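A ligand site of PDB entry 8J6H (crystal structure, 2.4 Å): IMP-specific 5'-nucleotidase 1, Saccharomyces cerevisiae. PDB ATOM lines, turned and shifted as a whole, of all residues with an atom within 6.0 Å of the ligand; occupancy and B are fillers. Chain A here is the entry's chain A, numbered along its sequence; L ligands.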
ATOM      1  N   ASP A  14      32.299   4.361  11.369  1.00  0.00           N
ATOM      2  CA  ASP A  14      31.973   3.033  11.880  1.00  0.00           C
ATOM      3  C   ASP A  14      31.457   2.140  10.755  1.00  0.00           C
ATOM      4  O   ASP A  14      30.413   2.410  10.161  1.00  0.00           O
ATOM      5  CB  ASP A  14      30.936   3.135  12.998  1.00  0.00           C
ATOM      6  CG  ASP A  14      30.777   1.831  13.759  1.00  0.00           C
ATOM      7  OD1 ASP A  14      31.456   1.659  14.790  1.00  0.00           O
ATOM      8  OD2 ASP A  14      29.963   0.990  13.321  1.00  0.00           O
ATOM      9  N   GLU A  15      32.183   1.063  10.477  1.00  0.00           N
ATOM     10  CA  GLU A  15      31.849   0.171   9.374  1.00  0.00           C
ATOM     11  C   GLU A  15      30.572  -0.619   9.639  1.00  0.00           C
ATOM     12  O   GLU A  15      29.811  -0.903   8.716  1.00  0.00           O
ATOM     13  CB  GLU A  15      32.999  -0.799   9.092  1.00  0.00           C
ATOM     14  CG  GLU A  15      32.904  -1.483   7.743  1.00  0.00           C
ATOM     15  CD  GLU A  15      33.735  -2.744   7.665  1.00  0.00           C
ATOM     16  OE1 GLU A  15      33.388  -3.633   6.856  1.00  0.00           O
ATOM     17  OE2 GLU A  15      34.721  -2.859   8.413  1.00  0.00           O
ATOM     18  N   PHE A  16      30.354  -0.991  10.900  1.00  0.00           N
ATOM     19  CA  PHE A  16      29.194  -1.786  11.275  1.00  0.00           C
ATOM     20  C   PHE A  16      27.891  -1.052  10.974  1.00  0.00           C
ATOM     21  O   PHE A  16      26.952  -1.638  10.436  1.00  0.00           O
ATOM     22  CB  PHE A  16      29.251  -2.161  12.756  1.00  0.00           C
ATOM     23  CG  PHE A  16      28.077  -2.973  13.221  1.00  0.00           C
ATOM     24  CD1 PHE A  16      27.349  -2.590  14.334  1.00  0.00           C
ATOM     25  CD2 PHE A  16      27.693  -4.122  12.538  1.00  0.00           C
ATOM     26  CE1 PHE A  16      26.269  -3.337  14.763  1.00  0.00           C
ATOM     27  CE2 PHE A  16      26.613  -4.869  12.967  1.00  0.00           C
ATOM     28  CZ  PHE A  16      25.897  -4.479  14.075  1.00  0.00           C
ATOM     29  N   ILE A  17      27.846   0.240  11.312  1.00  0.00           N
ATOM     30  CA  ILE A  17      26.660   1.053  11.053  1.00  0.00           C
ATOM     31  C   ILE A  17      26.415   1.211   9.560  1.00  0.00           C
ATOM     32  O   ILE A  17      25.277   1.115   9.090  1.00  0.00           O
ATOM     33  CB  ILE A  17      26.774   2.440  11.708  1.00  0.00           C
ATOM     34  CG1 ILE A  17      26.930   2.302  13.227  1.00  0.00           C
ATOM     35  CG2 ILE A  17      25.560   3.283  11.380  1.00  0.00           C
ATOM     36  CD1 ILE A  17      26.921   3.618  13.970  1.00  0.00           C
ATOM     37  N   VAL A 101      32.238  -7.768   8.492  1.00  0.00           N
ATOM     38  CA  VAL A 101      32.742  -6.490   8.974  1.00  0.00           C
ATOM     39  C   VAL A 101      34.056  -6.690   9.734  1.00  0.00           C
ATOM     40  O   VAL A 101      34.041  -7.013  10.922  1.00  0.00           O
ATOM     41  CB  VAL A 101      31.715  -5.785   9.897  1.00  0.00           C
ATOM     42  CG1 VAL A 101      32.183  -4.390  10.248  1.00  0.00           C
ATOM     43  CG2 VAL A 101      30.350  -5.761   9.243  1.00  0.00           C
ATOM     44  N   SER A 103      36.396  -4.571  10.693  1.00  0.00           N
ATOM     45  CA  SER A 103      36.768  -3.562  11.679  1.00  0.00           C
ATOM     46  C   SER A 103      35.772  -3.513  12.839  1.00  0.00           C
ATOM     47  O   SER A 103      35.705  -2.518  13.563  1.00  0.00           O
ATOM     48  CB  SER A 103      36.863  -2.181  11.023  1.00  0.00           C
ATOM     49  OG  SER A 103      35.576  -1.602  10.878  1.00  0.00           O
ATOM     50  N   ILE A 104      35.007  -4.588  13.013  1.00  0.00           N
ATOM     51  CA  ILE A 104      33.979  -4.618  14.040  1.00  0.00           C
ATOM     52  C   ILE A 104      34.604  -4.844  15.419  1.00  0.00           C
ATOM     53  O   ILE A 104      35.550  -5.606  15.574  1.00  0.00           O
ATOM     54  CB  ILE A 104      32.903  -5.698  13.741  1.00  0.00           C
ATOM     55  CG1 ILE A 104      31.615  -5.402  14.507  1.00  0.00           C
ATOM     56  CG2 ILE A 104      33.422  -7.100  14.042  1.00  0.00           C
ATOM     57  CD1 ILE A 104      30.398  -6.080  13.923  1.00  0.00           C
ATOM     58  N   GLY A 105      34.066  -4.143  16.418  1.00  0.00           N
ATOM     59  CA  GLY A 105      34.535  -4.284  17.776  1.00  0.00           C
ATOM     60  C   GLY A 105      33.836  -5.446  18.457  1.00  0.00           C
ATOM     61  O   GLY A 105      32.833  -5.947  17.953  1.00  0.00           O
ATOM     62  N   THR A 106      34.354  -5.871  19.596  1.00  0.00           N
ATOM     63  CA  THR A 106      33.764  -6.964  20.346  1.00  0.00           C
ATOM     64  C   THR A 106      32.477  -6.508  21.033  1.00  0.00           C
ATOM     65  O   THR A 106      32.392  -5.380  21.521  1.00  0.00           O
ATOM     66  CB  THR A 106      34.732  -7.541  21.394  1.00  0.00           C
ATOM     67  OG1 THR A 106      35.247  -6.469  22.202  1.00  0.00           O
ATOM     68  CG2 THR A 106      35.884  -8.248  20.713  1.00  0.00           C
ATOM     69  N   PHE A 107      31.489  -7.394  21.070  1.00  0.00           N
ATOM     70  CA  PHE A 107      30.233  -7.123  21.769  1.00  0.00           C
ATOM     71  C   PHE A 107      30.206  -7.847  23.103  1.00  0.00           C
ATOM     72  O   PHE A 107      30.028  -9.058  23.157  1.00  0.00           O
ATOM     73  CB  PHE A 107      29.032  -7.547  20.910  1.00  0.00           C
ATOM     74  CG  PHE A 107      28.887  -6.764  19.631  1.00  0.00           C
ATOM     75  CD1 PHE A 107      29.546  -7.159  18.483  1.00  0.00           C
ATOM     76  CD2 PHE A 107      28.078  -5.637  19.585  1.00  0.00           C
ATOM     77  CE1 PHE A 107      29.408  -6.445  17.310  1.00  0.00           C
ATOM     78  CE2 PHE A 107      27.943  -4.913  18.413  1.00  0.00           C
ATOM     79  CZ  PHE A 107      28.604  -5.321  17.272  1.00  0.00           C
ATOM     80  N   THR A 109      28.037  -7.380  25.432  1.00  0.00           N
ATOM     81  CA  THR A 109      26.663  -7.698  25.757  1.00  0.00           C
ATOM     82  C   THR A 109      25.842  -7.885  24.487  1.00  0.00           C
ATOM     83  O   THR A 109      26.136  -7.309  23.438  1.00  0.00           O
ATOM     84  CB  THR A 109      25.995  -6.617  26.617  1.00  0.00           C
ATOM     85  OG1 THR A 109      26.025  -5.357  25.921  1.00  0.00           O
ATOM     86  CG2 THR A 109      26.710  -6.473  27.950  1.00  0.00           C
ATOM     87  N   LEU A 111      22.441  -7.282  22.353  1.00  0.00           N
ATOM     88  CA  LEU A 111      21.611  -6.093  22.219  1.00  0.00           C
ATOM     89  C   LEU A 111      20.244  -6.468  21.654  1.00  0.00           C
ATOM     90  O   LEU A 111      20.145  -7.264  20.711  1.00  0.00           O
ATOM     91  CB  LEU A 111      22.299  -5.053  21.327  1.00  0.00           C
ATOM     92  CG  LEU A 111      23.742  -4.669  21.662  1.00  0.00           C
ATOM     93  CD1 LEU A 111      24.421  -4.060  20.446  1.00  0.00           C
ATOM     94  CD2 LEU A 111      23.777  -3.703  22.831  1.00  0.00           C
ATOM     95  N   ARG A 140      22.686   4.576  14.919  1.00  0.00           N
ATOM     96  CA  ARG A 140      23.424   4.931  16.129  1.00  0.00           C
ATOM     97  C   ARG A 140      22.476   5.089  17.311  1.00  0.00           C
ATOM     98  O   ARG A 140      22.764   4.617  18.415  1.00  0.00           O
ATOM     99  CB  ARG A 140      24.211   6.229  15.911  1.00  0.00           C
ATOM    100  CG  ARG A 140      24.996   6.684  17.128  1.00  0.00           C
ATOM    101  CD  ARG A 140      25.740   7.984  16.851  1.00  0.00           C
ATOM    102  NE  ARG A 140      24.834   9.074  16.531  1.00  0.00           N
ATOM    103  CZ  ARG A 140      24.357   9.937  17.427  1.00  0.00           C
ATOM    104  NH1 ARG A 140      24.701   9.832  18.704  1.00  0.00           N
ATOM    105  NH2 ARG A 140      23.539  10.914  17.047  1.00  0.00           N
ATOM    106  N   LEU A 143      21.196   1.582  18.183  1.00  0.00           N
ATOM    107  CA  LEU A 143      22.251   0.844  18.859  1.00  0.00           C
ATOM    108  C   LEU A 143      22.412   1.296  20.305  1.00  0.00           C
ATOM    109  O   LEU A 143      22.545   0.467  21.204  1.00  0.00           O
ATOM    110  CB  LEU A 143      23.567   1.000  18.105  1.00  0.00           C
ATOM    111  CG  LEU A 143      23.724   0.155  16.835  1.00  0.00           C
ATOM    112  CD1 LEU A 143      25.047   0.439  16.160  1.00  0.00           C
ATOM    113  CD2 LEU A 143      23.585  -1.330  17.160  1.00  0.00           C
ATOM    114  N   ASN A 144      22.405   2.610  20.528  1.00  0.00           N
ATOM    115  CA  ASN A 144      22.497   3.154  21.877  1.00  0.00           C
ATOM    116  C   ASN A 144      21.310   2.753  22.733  1.00  0.00           C
ATOM    117  O   ASN A 144      21.474   2.335  23.874  1.00  0.00           O
ATOM    118  CB  ASN A 144      22.605   4.683  21.823  1.00  0.00           C
ATOM    119  CG  ASN A 144      23.946   5.157  21.304  1.00  0.00           C
ATOM    120  OD1 ASN A 144      24.950   4.463  21.423  1.00  0.00           O
ATOM    121  ND2 ASN A 144      23.961   6.355  20.718  1.00  0.00           N
ATOM    122  N   GLN A 147      21.581  -0.815  23.884  1.00  0.00           N
ATOM    123  CA  GLN A 147      22.524  -1.041  24.965  1.00  0.00           C
ATOM    124  C   GLN A 147      21.907  -0.697  26.315  1.00  0.00           C
ATOM    125  O   GLN A 147      22.060  -1.425  27.288  1.00  0.00           O
ATOM    126  CB  GLN A 147      23.795  -0.222  24.751  1.00  0.00           C
ATOM    127  CG  GLN A 147      24.943  -0.604  25.671  1.00  0.00           C
ATOM    128  CD  GLN A 147      25.434  -2.028  25.439  1.00  0.00           C
ATOM    129  OE1 GLN A 147      26.226  -2.277  24.532  1.00  0.00           O
ATOM    130  NE2 GLN A 147      24.945  -2.962  26.245  1.00  0.00           N
ATOM    131  N   LEU A 404      29.796   0.824  31.066  1.00  0.00           N
ATOM    132  CA  LEU A 404      29.245   1.623  29.973  1.00  0.00           C
ATOM    133  C   LEU A 404      29.975   2.954  29.839  1.00  0.00           C
ATOM    134  O   LEU A 404      29.941   3.785  30.743  1.00  0.00           O
ATOM    135  CB  LEU A 404      27.759   1.870  30.178  1.00  0.00           C
ATOM    136  CG  LEU A 404      27.043   2.608  29.042  1.00  0.00           C
ATOM    137  CD1 LEU A 404      27.107   1.791  27.755  1.00  0.00           C
ATOM    138  CD2 LEU A 404      25.605   2.925  29.404  1.00  0.00           C
ATOM    139  N   ARG A 422      35.902   0.721  23.368  1.00  0.00           N
ATOM    140  CA  ARG A 422      35.135  -0.474  23.032  1.00  0.00           C
ATOM    141  C   ARG A 422      35.933  -1.737  23.344  1.00  0.00           C
ATOM    142  O   ARG A 422      35.376  -2.830  23.357  1.00  0.00           O
ATOM    143  CB  ARG A 422      34.732  -0.451  21.552  1.00  0.00           C
ATOM    144  CG  ARG A 422      33.645   0.549  21.213  1.00  0.00           C
ATOM    145  CD  ARG A 422      33.099   0.315  19.815  1.00  0.00           C
ATOM    146  NE  ARG A 422      32.082   1.291  19.461  1.00  0.00           N
ATOM    147  CZ  ARG A 422      31.793   1.661  18.221  1.00  0.00           C
ATOM    148  NH1 ARG A 422      32.453   1.132  17.196  1.00  0.00           N
ATOM    149  NH2 ARG A 422      30.843   2.552  17.991  1.00  0.00           N
ATOM    150  N   GLY A 425      34.918  -2.270  27.304  1.00  0.00           N
ATOM    151  CA  GLY A 425      33.533  -2.473  27.689  1.00  0.00           C
ATOM    152  C   GLY A 425      32.490  -1.922  26.740  1.00  0.00           C
ATOM    153  O   GLY A 425      32.821  -1.494  25.627  1.00  0.00           O
ATOM    154  N   CYS A 426      31.237  -1.934  27.174  1.00  0.00           N
ATOM    155  CA  CYS A 426      30.139  -1.392  26.380  1.00  0.00           C
ATOM    156  C   CYS A 426      30.272   0.123  26.279  1.00  0.00           C
ATOM    157  O   CYS A 426      30.869   0.758  27.148  1.00  0.00           O
ATOM    158  CB  CYS A 426      28.787  -1.754  26.995  1.00  0.00           C
ATOM    159  SG  CYS A 426      28.543  -3.525  27.257  1.00  0.00           S
ATOM    160  N   THR A 427      29.718   0.703  25.219  1.00  0.00           N
ATOM    161  CA  THR A 427      29.839   2.139  25.012  1.00  0.00           C
ATOM    162  C   THR A 427      28.549   2.791  24.537  1.00  0.00           C
ATOM    163  O   THR A 427      27.607   2.117  24.117  1.00  0.00           O
ATOM    164  CB  THR A 427      30.960   2.464  24.009  1.00  0.00           C
ATOM    165  OG1 THR A 427      31.437   3.794  24.243  1.00  0.00           O
ATOM    166  CG2 THR A 427      30.439   2.354  22.579  1.00  0.00           C
ATOM    167  N   LEU A 428      28.516   4.111  24.618  1.00  0.00           N
ATOM    168  CA  LEU A 428      27.383   4.906  24.160  1.00  0.00           C
ATOM    169  C   LEU A 428      27.901   6.053  23.290  1.00  0.00           C
ATOM    170  O   LEU A 428      28.709   6.871  23.748  1.00  0.00           O
ATOM    171  CB  LEU A 428      26.589   5.445  25.346  1.00  0.00           C
ATOM    172  CG  LEU A 428      25.080   5.194  25.372  1.00  0.00           C
ATOM    173  CD1 LEU A 428      24.777   3.701  25.303  1.00  0.00           C
ATOM    174  CD2 LEU A 428      24.468   5.807  26.620  1.00  0.00           C
ATOM    175  N   TRP A 429      27.440   6.101  22.052  1.00  0.00           N
ATOM    176  CA  TRP A 429      27.861   7.152  21.122  1.00  0.00           C
ATOM    177  C   TRP A 429      26.877   8.313  21.172  1.00  0.00           C
ATOM    178  O   TRP A 429      25.775   8.234  20.623  1.00  0.00           O
ATOM    179  CB  TRP A 429      27.964   6.584  19.703  1.00  0.00           C
ATOM    180  CG  TRP A 429      28.599   7.489  18.672  1.00  0.00           C
ATOM    181  CD1 TRP A 429      28.677   8.857  18.712  1.00  0.00           C
ATOM    182  CD2 TRP A 429      29.232   7.091  17.453  1.00  0.00           C
ATOM    183  NE1 TRP A 429      29.313   9.329  17.598  1.00  0.00           N
ATOM    184  CE2 TRP A 429      29.666   8.265  16.805  1.00  0.00           C
ATOM    185  CE3 TRP A 429      29.465   5.856  16.845  1.00  0.00           C
ATOM    186  CZ2 TRP A 429      30.326   8.235  15.579  1.00  0.00           C
ATOM    187  CZ3 TRP A 429      30.134   5.833  15.628  1.00  0.00           C
ATOM    188  CH2 TRP A 429      30.558   7.017  15.015  1.00  0.00           C
HETATM  189  N1  LIG L   1      30.064  -2.566  19.520  1.00  0.00           N
HETATM  190  C1  LIG L   1      29.832  -1.735  18.399  1.00  0.00           C
HETATM  191  N2  LIG L   1      28.952  -0.681  18.111  1.00  0.00           N
HETATM  192  C2  LIG L   1      28.955  -0.059  16.891  1.00  0.00           C
HETATM  193  N3  LIG L   1      29.839  -0.466  15.931  1.00  0.00           N
HETATM  194  C3  LIG L   1      30.698  -1.488  16.194  1.00  0.00           C
HETATM  195  O1  LIG L   1      31.574  -1.810  15.085  1.00  0.00           O
HETATM  196  C4  LIG L   1      30.685  -2.121  17.441  1.00  0.00           C
HETATM  197  N4  LIG L   1      31.451  -3.165  17.916  1.00  0.00           N
HETATM  198  C5  LIG L   1      31.053  -3.415  19.196  1.00  0.00           C
HETATM  199  C6  LIG L   1      26.097  -0.502  20.197  1.00  0.00           C
HETATM  200  O2  LIG L   1      26.648   0.777  19.909  1.00  0.00           O
HETATM  201  C7  LIG L   1      27.035  -1.343  21.033  1.00  0.00           C
HETATM  202  O3  LIG L   1      27.830  -2.192  20.165  1.00  0.00           O
HETATM  203  C8  LIG L   1      29.155  -2.197  20.618  1.00  0.00           C
HETATM  204  C9  LIG L   1      29.373  -0.811  21.207  1.00  0.00           C
HETATM  205  O4  LIG L   1      30.500  -0.779  22.069  1.00  0.00           O
HETATM  206  C10 LIG L   1      28.036  -0.552  21.903  1.00  0.00           C
HETATM  207  O5  LIG L   1      28.068  -1.102  23.214  1.00  0.00           O
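The side-chain amide oxygen (OE1) of Gln 147 sits at hydrogen-bond distance from an oxygen (O5) of the ligand (2.6 Å). The side-chain carboxylate (OD1) of Asp 14 sits at hydrogen-bond distance from a nitrogen (N3) of the ligand, at 2.9 Å. The backbone NH of Gly 105 sits at hydrogen-bond distance from a nitrogen (N4) of the ligand (3.2 Å). The backbone NH of Thr 427 sits at hydrogen-bond distance from an oxygen (O5) of the ligand, 3.2 Å away. An oxygen (O5) of the ligand sits at hydrogen-bond distance from the backbone carbonyl oxygen (O) of Thr 427.
NH1 of Arg 422 sits close to N3 of the ligand, at 3.3 Å. Phe 16 touches the ligand (CB to O1, 3.3 Å). Ile 104 touches the ligand (CG1 to O1, 3.6 Å). O of Thr 106 touches C5 of the ligand (3.3 Å). Phe 107 touches the ligand (CE2 to O3, 3.2 Å). CD1 of Leu 111 touches C7 of the ligand (3.8 Å). Leu 143 touches the ligand. Cys 426 touches the ligand. 12 residues have an atom within 4 Å of the ligand: Asp 14, Phe 16, Ile 104, Gly 105, Thr 106, Phe 107, Leu 111, Leu 143, Gln 147, Arg 422, Cys 426 and Thr 427.
The side-chain sulfur (SG) of Cys 426 sits at hydrogen-bond distance from the side-chain amide nitrogen (NE2) of Gln 147 (3.8 Å). OG1 of Thr 109 is in hydrogen-bond range of NE2 of Gln 147, at 2.6 Å. The backbone NH of Phe 16 sits at hydrogen-bond distance from the side-chain carboxylate of Asp 14 (3.2 Å). The guanidinium group (NH1) of Arg 422 is in salt-bridge range of the side-chain carboxylate (OD1) of Asp 14 (2.7 Å). OD2 of Asp 14 lies within hydrogen-bond range of N of Ile 17 (3.0 Å). SG of Cys 426 lies within hydrogen-bond range of OG1 of Thr 109, 3.4 Å away.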
